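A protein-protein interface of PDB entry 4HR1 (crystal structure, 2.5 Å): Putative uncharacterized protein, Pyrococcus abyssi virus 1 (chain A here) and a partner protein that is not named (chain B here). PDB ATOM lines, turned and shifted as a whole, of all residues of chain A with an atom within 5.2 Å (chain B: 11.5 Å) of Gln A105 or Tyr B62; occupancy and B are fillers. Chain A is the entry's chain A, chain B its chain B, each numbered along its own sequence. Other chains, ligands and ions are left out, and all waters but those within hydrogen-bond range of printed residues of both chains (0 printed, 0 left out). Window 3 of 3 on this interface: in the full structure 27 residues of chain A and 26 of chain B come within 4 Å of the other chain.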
ATOM      1  N   PHE A  22      23.871  -1.398  19.204  1.00  0.00           N
ATOM      2  CA  PHE A  22      23.085  -2.350  18.412  1.00  0.00           C
ATOM      3  C   PHE A  22      23.130  -2.008  16.928  1.00  0.00           C
ATOM      4  O   PHE A  22      23.462  -2.882  16.122  1.00  0.00           O
ATOM      5  CB  PHE A  22      21.636  -2.392  18.926  1.00  0.00           C
ATOM      6  CG  PHE A  22      20.747  -3.444  18.308  1.00  0.00           C
ATOM      7  CD1 PHE A  22      20.061  -3.194  17.126  1.00  0.00           C
ATOM      8  CD2 PHE A  22      20.546  -4.664  18.940  1.00  0.00           C
ATOM      9  CE1 PHE A  22      19.219  -4.158  16.569  1.00  0.00           C
ATOM     10  CE2 PHE A  22      19.687  -5.617  18.391  1.00  0.00           C
ATOM     11  CZ  PHE A  22      19.024  -5.356  17.214  1.00  0.00           C
ATOM     12  N   ALA A 102      14.594  -5.074  11.434  1.00  0.00           N
ATOM     13  CA  ALA A 102      13.205  -5.468  11.705  1.00  0.00           C
ATOM     14  C   ALA A 102      12.341  -5.528  10.417  1.00  0.00           C
ATOM     15  O   ALA A 102      11.267  -4.916  10.334  1.00  0.00           O
ATOM     16  CB  ALA A 102      12.588  -4.552  12.754  1.00  0.00           C
ATOM     17  N   GLN A 103      12.838  -6.277   9.407  1.00  0.00           N
ATOM     18  CA  GLN A 103      12.201  -6.440   8.097  1.00  0.00           C
ATOM     19  C   GLN A 103      10.903  -7.227   8.217  1.00  0.00           C
ATOM     20  O   GLN A 103       9.827  -6.674   7.966  1.00  0.00           O
ATOM     21  CB  GLN A 103      13.172  -7.102   7.103  1.00  0.00           C
ATOM     22  CG  GLN A 103      12.945  -6.684   5.660  1.00  0.00           C
ATOM     23  CD  GLN A 103      13.509  -5.316   5.383  1.00  0.00           C
ATOM     24  OE1 GLN A 103      14.730  -5.118   5.339  1.00  0.00           O
ATOM     25  NE2 GLN A 103      12.631  -4.340   5.194  1.00  0.00           N
ATOM     26  N   GLY A 104      11.026  -8.495   8.614  1.00  0.00           N
ATOM     27  CA  GLY A 104       9.907  -9.399   8.851  1.00  0.00           C
ATOM     28  C   GLY A 104       9.647  -9.465  10.341  1.00  0.00           C
ATOM     29  O   GLY A 104       9.800 -10.523  10.963  1.00  0.00           O
ATOM     30  N   GLN A 105       9.304  -8.303  10.921  1.00  0.00           N
ATOM     31  CA  GLN A 105       9.049  -8.098  12.347  1.00  0.00           C
ATOM     32  C   GLN A 105       7.965  -7.020  12.482  1.00  0.00           C
ATOM     33  O   GLN A 105       7.948  -6.073  11.681  1.00  0.00           O
ATOM     34  CB  GLN A 105      10.368  -7.645  13.030  1.00  0.00           C
ATOM     35  CG  GLN A 105      10.356  -7.527  14.567  1.00  0.00           C
ATOM     36  CD  GLN A 105      11.693  -7.073  15.150  1.00  0.00           C
ATOM     37  OE1 GLN A 105      12.773  -7.608  14.841  1.00  0.00           O
ATOM     38  NE2 GLN A 105      11.652  -6.099  16.038  1.00  0.00           N
ATOM     39  N   MET A 106       7.061  -7.177  13.486  1.00  0.00           N
ATOM     40  CA  MET A 106       5.983  -6.237  13.820  1.00  0.00           C
ATOM     41  C   MET A 106       6.649  -4.968  14.420  1.00  0.00           C
ATOM     42  O   MET A 106       6.895  -4.884  15.635  1.00  0.00           O
ATOM     43  CB  MET A 106       4.996  -6.890  14.817  1.00  0.00           C
ATOM     44  CG  MET A 106       3.548  -6.464  14.611  1.00  0.00           C
ATOM     45  SD  MET A 106       2.591  -6.221  16.140  1.00  0.00           S
ATOM     46  CE  MET A 106       2.473  -7.923  16.759  1.00  0.00           C
ATOM     47  N   GLY A 107       6.997  -4.036  13.533  1.00  0.00           N
ATOM     48  CA  GLY A 107       7.711  -2.818  13.887  1.00  0.00           C
ATOM     49  C   GLY A 107       9.089  -3.139  14.423  1.00  0.00           C
ATOM     50  O   GLY A 107       9.823  -3.897  13.799  1.00  0.00           O
ATOM     51  N   THR A 108       9.430  -2.611  15.600  1.00  0.00           N
ATOM     52  CA  THR A 108      10.718  -2.878  16.253  1.00  0.00           C
ATOM     53  C   THR A 108      10.482  -3.505  17.615  1.00  0.00           C
ATOM     54  O   THR A 108      11.349  -3.429  18.477  1.00  0.00           O
ATOM     55  CB  THR A 108      11.568  -1.589  16.377  1.00  0.00           C
ATOM     56  OG1 THR A 108      10.827  -0.613  17.111  1.00  0.00           O
ATOM     57  CG2 THR A 108      12.027  -1.035  15.038  1.00  0.00           C
ATOM     58  N   LEU A 109       9.319  -4.121  17.811  1.00  0.00           N
ATOM     59  CA  LEU A 109       8.902  -4.735  19.067  1.00  0.00           C
ATOM     60  C   LEU A 109       9.871  -5.715  19.700  1.00  0.00           C
ATOM     61  O   LEU A 109      10.051  -5.669  20.918  1.00  0.00           O
ATOM     62  CB  LEU A 109       7.541  -5.408  18.903  1.00  0.00           C
ATOM     63  CG  LEU A 109       6.338  -4.671  19.477  1.00  0.00           C
ATOM     64  CD1 LEU A 109       5.051  -5.370  19.054  1.00  0.00           C
ATOM     65  CD2 LEU A 109       6.405  -4.574  21.017  1.00  0.00           C
ATOM     66  N   LYS A 110      10.446  -6.632  18.901  1.00  0.00           N
ATOM     67  CA  LYS A 110      11.379  -7.634  19.425  1.00  0.00           C
ATOM     68  C   LYS A 110      12.738  -6.995  19.785  1.00  0.00           C
ATOM     69  O   LYS A 110      13.320  -7.344  20.812  1.00  0.00           O
ATOM     70  CB  LYS A 110      11.589  -8.783  18.425  1.00  0.00           C
ATOM     71  CG  LYS A 110      10.352  -9.610  18.097  1.00  0.00           C
ATOM     72  CD  LYS A 110      10.735 -10.796  17.195  1.00  0.00           C
ATOM     73  CE  LYS A 110       9.543 -11.510  16.606  1.00  0.00           C
ATOM     74  NZ  LYS A 110       9.961 -12.679  15.786  1.00  0.00           N
ATOM     75  N   ILE A 111      13.234  -6.081  18.916  1.00  0.00           N
ATOM     76  CA  ILE A 111      14.491  -5.363  19.072  1.00  0.00           C
ATOM     77  C   ILE A 111      14.398  -4.560  20.353  1.00  0.00           C
ATOM     78  O   ILE A 111      15.289  -4.659  21.205  1.00  0.00           O
ATOM     79  CB  ILE A 111      14.772  -4.443  17.842  1.00  0.00           C
ATOM     80  CG1 ILE A 111      15.234  -5.257  16.618  1.00  0.00           C
ATOM     81  CG2 ILE A 111      15.769  -3.322  18.189  1.00  0.00           C
ATOM     82  CD1 ILE A 111      15.227  -4.495  15.384  1.00  0.00           C
ATOM     83  N   TYR A 114      14.415  -6.767  23.484  1.00  0.00           N
ATOM     84  CA  TYR A 114      15.796  -7.197  23.663  1.00  0.00           C
ATOM     85  C   TYR A 114      16.623  -6.055  24.296  1.00  0.00           C
ATOM     86  O   TYR A 114      17.309  -6.279  25.288  1.00  0.00           O
ATOM     87  CB  TYR A 114      16.402  -7.645  22.321  1.00  0.00           C
ATOM     88  CG  TYR A 114      17.905  -7.809  22.355  1.00  0.00           C
ATOM     89  CD1 TYR A 114      18.497  -8.848  23.072  1.00  0.00           C
ATOM     90  CD2 TYR A 114      18.738  -6.940  21.654  1.00  0.00           C
ATOM     91  CE1 TYR A 114      19.880  -8.998  23.115  1.00  0.00           C
ATOM     92  CE2 TYR A 114      20.121  -7.085  21.683  1.00  0.00           C
ATOM     93  CZ  TYR A 114      20.690  -8.119  22.416  1.00  0.00           C
ATOM     94  OH  TYR A 114      22.060  -8.252  22.473  1.00  0.00           O
ATOM     95  N   ASN B   4      27.247 -13.490  31.357  1.00  0.00           N
ATOM     96  CA  ASN B   4      26.045 -13.910  30.649  1.00  0.00           C
ATOM     97  C   ASN B   4      25.824 -13.225  29.286  1.00  0.00           C
ATOM     98  O   ASN B   4      24.705 -13.232  28.771  1.00  0.00           O
ATOM     99  CB  ASN B   4      24.824 -13.764  31.566  1.00  0.00           C
ATOM    100  CG  ASN B   4      24.548 -12.357  32.033  1.00  0.00           C
ATOM    101  OD1 ASN B   4      24.367 -11.432  31.237  1.00  0.00           O
ATOM    102  ND2 ASN B   4      24.477 -12.171  33.344  1.00  0.00           N
ATOM    103  N   GLY B   5      26.874 -12.645  28.721  1.00  0.00           N
ATOM    104  CA  GLY B   5      26.808 -11.983  27.425  1.00  0.00           C
ATOM    105  C   GLY B   5      26.658 -10.474  27.485  1.00  0.00           C
ATOM    106  O   GLY B   5      27.202  -9.826  28.388  1.00  0.00           O
ATOM    107  N   ALA B   6      25.887  -9.914  26.523  1.00  0.00           N
ATOM    108  CA  ALA B   6      25.603  -8.489  26.346  1.00  0.00           C
ATOM    109  C   ALA B   6      25.102  -7.772  27.602  1.00  0.00           C
ATOM    110  O   ALA B   6      25.558  -6.663  27.864  1.00  0.00           O
ATOM    111  CB  ALA B   6      24.645  -8.279  25.192  1.00  0.00           C
ATOM    112  N   GLN B   7      24.232  -8.413  28.403  1.00  0.00           N
ATOM    113  CA  GLN B   7      23.697  -7.821  29.634  1.00  0.00           C
ATOM    114  C   GLN B   7      24.817  -7.467  30.609  1.00  0.00           C
ATOM    115  O   GLN B   7      24.802  -6.355  31.132  1.00  0.00           O
ATOM    116  CB  GLN B   7      22.636  -8.719  30.295  1.00  0.00           C
ATOM    117  CG  GLN B   7      21.893  -8.056  31.454  1.00  0.00           C
ATOM    118  CD  GLN B   7      21.939  -8.895  32.706  1.00  0.00           C
ATOM    119  OE1 GLN B   7      21.029  -9.681  32.982  1.00  0.00           O
ATOM    120  NE2 GLN B   7      22.993  -8.743  33.504  1.00  0.00           N
ATOM    121  N   VAL B   9      28.143  -6.916  29.983  1.00  0.00           N
ATOM    122  CA  VAL B   9      28.919  -5.840  29.366  1.00  0.00           C
ATOM    123  C   VAL B   9      28.235  -4.473  29.461  1.00  0.00           C
ATOM    124  O   VAL B   9      28.898  -3.513  29.848  1.00  0.00           O
ATOM    125  CB  VAL B   9      29.491  -6.164  27.946  1.00  0.00           C
ATOM    126  CG1 VAL B   9      29.927  -7.620  27.837  1.00  0.00           C
ATOM    127  CG2 VAL B   9      28.515  -5.812  26.828  1.00  0.00           C
ATOM    128  N   ILE B  10      26.914  -4.399  29.137  1.00  0.00           N
ATOM    129  CA  ILE B  10      26.121  -3.171  29.205  1.00  0.00           C
ATOM    130  C   ILE B  10      26.041  -2.705  30.657  1.00  0.00           C
ATOM    131  O   ILE B  10      26.305  -1.530  30.934  1.00  0.00           O
ATOM    132  CB  ILE B  10      24.721  -3.310  28.506  1.00  0.00           C
ATOM    133  CG1 ILE B  10      24.840  -3.473  26.962  1.00  0.00           C
ATOM    134  CG2 ILE B  10      23.701  -2.204  28.904  1.00  0.00           C
ATOM    135  CD1 ILE B  10      25.639  -2.380  26.150  1.00  0.00           C
ATOM    136  N   VAL B  54      33.748  -3.946  22.428  1.00  0.00           N
ATOM    137  CA  VAL B  54      32.805  -4.941  22.929  1.00  0.00           C
ATOM    138  C   VAL B  54      31.331  -4.751  22.426  1.00  0.00           C
ATOM    139  O   VAL B  54      30.455  -5.568  22.741  1.00  0.00           O
ATOM    140  CB  VAL B  54      32.982  -5.031  24.468  1.00  0.00           C
ATOM    141  CG1 VAL B  54      31.922  -4.262  25.241  1.00  0.00           C
ATOM    142  CG2 VAL B  54      33.065  -6.467  24.930  1.00  0.00           C
ATOM    143  N   ASN B  55      31.096  -3.697  21.603  1.00  0.00           N
ATOM    144  CA  ASN B  55      29.785  -3.320  21.060  1.00  0.00           C
ATOM    145  C   ASN B  55      29.164  -4.330  20.137  1.00  0.00           C
ATOM    146  O   ASN B  55      27.935  -4.466  20.167  1.00  0.00           O
ATOM    147  CB  ASN B  55      29.818  -1.939  20.375  1.00  0.00           C
ATOM    148  CG  ASN B  55      29.653  -0.748  21.305  1.00  0.00           C
ATOM    149  OD1 ASN B  55      29.200  -0.853  22.471  1.00  0.00           O
ATOM    150  ND2 ASN B  55      30.017   0.420  20.792  1.00  0.00           N
ATOM    151  N   TRP B  56      29.996  -5.021  19.312  1.00  0.00           N
ATOM    152  CA  TRP B  56      29.586  -6.039  18.330  1.00  0.00           C
ATOM    153  C   TRP B  56      28.641  -7.082  18.947  1.00  0.00           C
ATOM    154  O   TRP B  56      27.727  -7.544  18.269  1.00  0.00           O
ATOM    155  CB  TRP B  56      30.819  -6.733  17.681  1.00  0.00           C
ATOM    156  CG  TRP B  56      31.750  -7.344  18.693  1.00  0.00           C
ATOM    157  CD1 TRP B  56      32.818  -6.740  19.282  1.00  0.00           C
ATOM    158  CD2 TRP B  56      31.624  -8.633  19.317  1.00  0.00           C
ATOM    159  NE1 TRP B  56      33.343  -7.551  20.261  1.00  0.00           N
ATOM    160  CE2 TRP B  56      32.610  -8.707  20.325  1.00  0.00           C
ATOM    161  CE3 TRP B  56      30.763  -9.731  19.131  1.00  0.00           C
ATOM    162  CZ2 TRP B  56      32.781  -9.843  21.125  1.00  0.00           C
ATOM    163  CZ3 TRP B  56      30.873 -10.816  19.987  1.00  0.00           C
ATOM    164  CH2 TRP B  56      31.892 -10.879  20.951  1.00  0.00           C
ATOM    165  N   ASP B  57      28.862  -7.420  20.234  1.00  0.00           N
ATOM    166  CA  ASP B  57      28.120  -8.401  21.021  1.00  0.00           C
ATOM    167  C   ASP B  57      26.656  -8.015  21.285  1.00  0.00           C
ATOM    168  O   ASP B  57      25.831  -8.908  21.528  1.00  0.00           O
ATOM    169  CB  ASP B  57      28.882  -8.716  22.329  1.00  0.00           C
ATOM    170  CG  ASP B  57      28.330  -9.879  23.145  1.00  0.00           C
ATOM    171  OD1 ASP B  57      28.139  -9.707  24.377  1.00  0.00           O
ATOM    172  OD2 ASP B  57      28.023 -10.939  22.543  1.00  0.00           O
ATOM    173  N   VAL B  58      26.340  -6.700  21.258  1.00  0.00           N
ATOM    174  CA  VAL B  58      24.971  -6.195  21.441  1.00  0.00           C
ATOM    175  C   VAL B  58      24.132  -6.714  20.273  1.00  0.00           C
ATOM    176  O   VAL B  58      23.132  -7.389  20.515  1.00  0.00           O
ATOM    177  CB  VAL B  58      24.845  -4.648  21.635  1.00  0.00           C
ATOM    178  CG1 VAL B  58      23.381  -4.216  21.701  1.00  0.00           C
ATOM    179  CG2 VAL B  58      25.574  -4.192  22.893  1.00  0.00           C
ATOM    180  N   TYR B  59      24.561  -6.459  19.027  1.00  0.00           N
ATOM    181  CA  TYR B  59      23.830  -6.987  17.882  1.00  0.00           C
ATOM    182  C   TYR B  59      24.009  -8.512  17.725  1.00  0.00           C
ATOM    183  O   TYR B  59      23.035  -9.186  17.377  1.00  0.00           O
ATOM    184  CB  TYR B  59      24.190  -6.275  16.586  1.00  0.00           C
ATOM    185  CG  TYR B  59      23.512  -6.908  15.394  1.00  0.00           C
ATOM    186  CD1 TYR B  59      22.163  -6.681  15.132  1.00  0.00           C
ATOM    187  CD2 TYR B  59      24.193  -7.811  14.579  1.00  0.00           C
ATOM    188  CE1 TYR B  59      21.519  -7.301  14.065  1.00  0.00           C
ATOM    189  CE2 TYR B  59      23.560  -8.435  13.507  1.00  0.00           C
ATOM    190  CZ  TYR B  59      22.222  -8.174  13.253  1.00  0.00           C
ATOM    191  OH  TYR B  59      21.593  -8.767  12.190  1.00  0.00           O
ATOM    192  N   ALA B  60      25.239  -9.044  17.966  1.00  0.00           N
ATOM    193  CA  ALA B  60      25.544 -10.475  17.832  1.00  0.00           C
ATOM    194  C   ALA B  60      24.669 -11.362  18.719  1.00  0.00           C
ATOM    195  O   ALA B  60      24.052 -12.278  18.198  1.00  0.00           O
ATOM    196  CB  ALA B  60      27.021 -10.749  18.075  1.00  0.00           C
ATOM    197  N   GLN B  61      24.530 -11.050  20.014  1.00  0.00           N
ATOM    198  CA  GLN B  61      23.678 -11.838  20.906  1.00  0.00           C
ATOM    199  C   GLN B  61      22.233 -11.901  20.388  1.00  0.00           C
ATOM    200  O   GLN B  61      21.576 -12.930  20.553  1.00  0.00           O
ATOM    201  CB  GLN B  61      23.718 -11.287  22.341  1.00  0.00           C
ATOM    202  CG  GLN B  61      22.933 -12.140  23.333  1.00  0.00           C
ATOM    203  CD  GLN B  61      23.354 -11.980  24.764  1.00  0.00           C
ATOM    204  OE1 GLN B  61      22.517 -11.874  25.671  1.00  0.00           O
ATOM    205  NE2 GLN B  61      24.652 -12.052  25.018  1.00  0.00           N
ATOM    206  N   TYR B  62      21.759 -10.803  19.754  1.00  0.00           N
ATOM    207  CA  TYR B  62      20.423 -10.675  19.199  1.00  0.00           C
ATOM    208  C   TYR B  62      20.267 -11.566  17.963  1.00  0.00           C
ATOM    209  O   TYR B  62      19.277 -12.300  17.850  1.00  0.00           O
ATOM    210  CB  TYR B  62      20.142  -9.203  18.830  1.00  0.00           C
ATOM    211  CG  TYR B  62      18.782  -9.018  18.209  1.00  0.00           C
ATOM    212  CD1 TYR B  62      17.626  -9.088  18.982  1.00  0.00           C
ATOM    213  CD2 TYR B  62      18.639  -8.838  16.839  1.00  0.00           C
ATOM    214  CE1 TYR B  62      16.365  -8.969  18.409  1.00  0.00           C
ATOM    215  CE2 TYR B  62      17.377  -8.716  16.252  1.00  0.00           C
ATOM    216  CZ  TYR B  62      16.245  -8.783  17.044  1.00  0.00           C
ATOM    217  OH  TYR B  62      14.996  -8.673  16.483  1.00  0.00           O
ATOM    218  N   ALA B  63      21.235 -11.453  17.023  1.00  0.00           N
ATOM    219  CA  ALA B  63      21.308 -12.193  15.772  1.00  0.00           C
ATOM    220  C   ALA B  63      21.292 -13.737  15.970  1.00  0.00           C
ATOM    221  O   ALA B  63      21.149 -14.471  14.985  1.00  0.00           O
ATOM    222  CB  ALA B  63      22.544 -11.766  15.005  1.00  0.00           C
ATOM    223  N   ARG B  64      21.428 -14.215  17.240  1.00  0.00           N
ATOM    224  CA  ARG B  64      21.409 -15.629  17.615  1.00  0.00           C
ATOM    225  C   ARG B  64      20.485 -15.975  18.786  1.00  0.00           C
ATOM    226  O   ARG B  64      20.913 -16.585  19.772  1.00  0.00           O
ATOM    227  CB  ARG B  64      22.814 -16.256  17.725  1.00  0.00           C
ATOM    228  CG  ARG B  64      23.873 -15.489  18.498  1.00  0.00           C
ATOM    229  CD  ARG B  64      25.015 -15.101  17.562  1.00  0.00           C
ATOM    230  NE  ARG B  64      26.324 -15.224  18.205  1.00  0.00           N
ATOM    231  CZ  ARG B  64      27.497 -15.049  17.593  1.00  0.00           C
ATOM    232  NH1 ARG B  64      27.543 -14.703  16.311  1.00  0.00           N
ATOM    233  NH2 ARG B  64      28.632 -15.233  18.256  1.00  0.00           N
ATOM    234  N   GLY B  65      19.221 -15.581  18.644  1.00  0.00           N
ATOM    235  CA  GLY B  65      18.126 -15.849  19.572  1.00  0.00           C
ATOM    236  C   GLY B  65      18.283 -15.432  21.018  1.00  0.00           C
ATOM    237  O   GLY B  65      17.666 -16.047  21.903  1.00  0.00           O
ATOM    238  N   ASP B  66      19.049 -14.348  21.274  1.00  0.00           N
ATOM    239  CA  ASP B  66      19.308 -13.850  22.629  1.00  0.00           C
ATOM    240  C   ASP B  66      19.914 -14.964  23.501  1.00  0.00           C
ATOM    241  O   ASP B  66      19.429 -15.321  24.579  1.00  0.00           O
ATOM    242  CB  ASP B  66      18.098 -13.103  23.264  1.00  0.00           C
ATOM    243  CG  ASP B  66      18.414 -12.390  24.577  1.00  0.00           C
ATOM    244  OD1 ASP B  66      17.472 -12.151  25.370  1.00  0.00           O
ATOM    245  OD2 ASP B  66      19.609 -12.096  24.827  1.00  0.00           O
ATOM    246  N   PHE B  67      20.960 -15.552  22.953  1.00  0.00           N
ATOM    247  CA  PHE B  67      21.745 -16.594  23.581  1.00  0.00           C
ATOM    248  C   PHE B  67      23.181 -16.130  23.528  1.00  0.00           C
ATOM    249  O   PHE B  67      23.645 -15.650  22.490  1.00  0.00           O
ATOM    250  CB  PHE B  67      21.604 -17.939  22.830  1.00  0.00           C
ATOM    251  CG  PHE B  67      20.243 -18.598  22.865  1.00  0.00           C
ATOM    252  CD1 PHE B  67      19.631 -18.913  24.079  1.00  0.00           C
ATOM    253  CD2 PHE B  67      19.596 -18.958  21.685  1.00  0.00           C
ATOM    254  CE1 PHE B  67      18.371 -19.532  24.110  1.00  0.00           C
ATOM    255  CE2 PHE B  67      18.345 -19.590  21.716  1.00  0.00           C
ATOM    256  CZ  PHE B  67      17.740 -19.869  22.928  1.00  0.00           C
ATOM    257  N   ASN B  68      23.875 -16.250  24.652  1.00  0.00           N
ATOM    258  CA  ASN B  68      25.281 -15.922  24.736  1.00  0.00           C
ATOM    259  C   ASN B  68      26.004 -17.171  24.206  1.00  0.00           C
ATOM    260  O   ASN B  68      26.244 -18.123  24.940  1.00  0.00           O
ATOM    261  CB  ASN B  68      25.669 -15.583  26.185  1.00  0.00           C
ATOM    262  CG  ASN B  68      27.158 -15.496  26.396  1.00  0.00           C
ATOM    263  OD1 ASN B  68      27.881 -14.798  25.674  1.00  0.00           O
ATOM    264  ND2 ASN B  68      27.649 -16.234  27.369  1.00  0.00           N
ATOM    265  N   LEU B  69      26.257 -17.174  22.906  1.00  0.00           N
ATOM    266  CA  LEU B  69      26.891 -18.237  22.142  1.00  0.00           C
ATOM    267  C   LEU B  69      27.998 -17.555  21.383  1.00  0.00           C
ATOM    268  O   LEU B  69      27.740 -16.777  20.469  1.00  0.00           O
ATOM    269  CB  LEU B  69      25.843 -18.837  21.179  1.00  0.00           C
ATOM    270  CG  LEU B  69      25.238 -20.233  21.454  1.00  0.00           C
ATOM    271  CD1 LEU B  69      25.301 -20.672  22.939  1.00  0.00           C
ATOM    272  CD2 LEU B  69      23.822 -20.303  20.920  1.00  0.00           C
ATOM    273  N   LEU B  70      29.231 -17.763  21.836  1.00  0.00           N
ATOM    274  CA  LEU B  70      30.420 -17.083  21.319  1.00  0.00           C
ATOM    275  C   LEU B  70      31.461 -18.026  20.757  1.00  0.00           C
ATOM    276  O   LEU B  70      31.671 -19.111  21.296  1.00  0.00           O
ATOM    277  CB  LEU B  70      31.046 -16.308  22.498  1.00  0.00           C
ATOM    278  CG  LEU B  70      30.816 -14.792  22.648  1.00  0.00           C
ATOM    279  CD1 LEU B  70      29.396 -14.365  22.278  1.00  0.00           C
ATOM    280  CD2 LEU B  70      31.155 -14.339  24.071  1.00  0.00           C
ATOM    281  N   GLU B  74      35.883 -14.502  19.837  1.00  0.00           N
ATOM    282  CA  GLU B  74      34.879 -13.737  20.564  1.00  0.00           C
ATOM    283  C   GLU B  74      34.983 -13.890  22.061  1.00  0.00           C
ATOM    284  O   GLU B  74      34.987 -12.874  22.756  1.00  0.00           O
ATOM    285  CB  GLU B  74      33.473 -14.103  20.102  1.00  0.00           C
ATOM    286  CG  GLU B  74      33.116 -13.475  18.776  1.00  0.00           C
ATOM    287  CD  GLU B  74      31.978 -14.171  18.072  1.00  0.00           C
ATOM    288  OE1 GLU B  74      31.302 -15.008  18.713  1.00  0.00           O
ATOM    289  OE2 GLU B  74      31.813 -13.936  16.855  1.00  0.00           O
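OH of Tyr B62 lies within hydrogen-bond range of OE1 of Gln A105. OH of Tyr A114 sits close to O of Val B58, 2.4 Å away.
NE2 of Gln A105 sits close to N of Lys A110, at 3.2 Å. The side-chain amide nitrogen (NE2) of Gln A105 lies close to the backbone NH (N) of Ile A111 (3.3 Å). The backbone NH of Ala B6 lies within hydrogen-bond range of the side-chain carboxylate of Asp B57, at 3.1 Å. The side-chain amide nitrogen (NE2) of Gln B61 lies close to the backbone NH (N) of Ala B6, at 2.9 Å. The backbone carbonyl oxygen of Gln B61 lies within hydrogen-bond range of the backbone NH of Asp B66 (3.0 Å).
Phe A22 touches Val B58 (CB to CG1, 3.8 Å). Tyr B59 touches Phe A22 (CB to O, 3.5 Å). Phe A22 touches Tyr B62 (CZ to CD2, 3.5 Å). Lys A110 touches Tyr B62 (CB to OH, 3.9 Å). OH of Tyr B62 touches CG1 of Ile A111 (3.4 Å). CB of Ala B6 touches OH of Tyr A114, at 3.8 Å. OH of Tyr A114 touches O of Asp B57, 3.9 Å away. OH of Tyr A114 touches CB of Gln B61, 3.5 Å away. Tyr B62 touches Tyr A114. CE1 of Tyr A114 touches OD2 of Asp B66, at 3.5 Å.
Gln A103 touches none of the printed residues of chain B. No residue of chain B comes within 4 Å of Gly A104. No residue of chain B comes within 4 Å of Met A106. No residue of chain B comes within 4 Å of Thr A108. No residue of chain B comes within 4 Å of Leu A109. Of chain B, only Tyr B62 (3.4 Å) comes within 4 Å of Ile A111. Printed residues of chain A within 4 Å of Asp B57: Tyr A114 (3.9 Å). Ala B60 touches none of the printed residues of chain A. Of the printed residues of chain A, Gln B61 touches Tyr A114. Tyr B62 touches just these residues of chain A: Phe A22 (3.5 Å), Gln A105 (3.0 Å), Lys A110 (3.9 Å), Ile A111 (3.4 Å) and Tyr A114 (3.6 Å). The nearest residue of chain B that does not touch Gln A105 is Tyr B59 (8.8 Å). The nearest printed residue of chain A that does not touch Tyr B62 is Ala A102 (6.0 Å). The nearest printed residue of chain B that does not touch Phe A22 is Asn B55 (5.2 Å).
Of the 12 printed residues of chain A, 5 touch a printed residue of chain B. Printed residues of chain A that touch a printed residue of chain B: Phe A22, Gln A105, Lys A110, Ile A111 and Tyr A114. Hydrophobic or aromatic side chains of chain A that line the printed part of chain B: Phe A22, Ile A111 and Tyr A114. Of the 24 printed residues of chain B, 7 touch a printed residue of chain A. Printed residues of chain B that touch a printed residue of chain A: Ala B6, Asp B57, Val B58, Tyr B59, Gln B61, Tyr B62 and Asp B66. Hydrophobic or aromatic side chains of chain B within 4 Å of the printed part of chain A: Ala B6, Val B58, Tyr B59 and Tyr B62. Among the printed residues, 12 pairs touch across the chains. Among the printed residues, no Asp or Glu carboxylate lies within 4 Å of a Lys or Arg side-chain nitrogen of the other chain.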
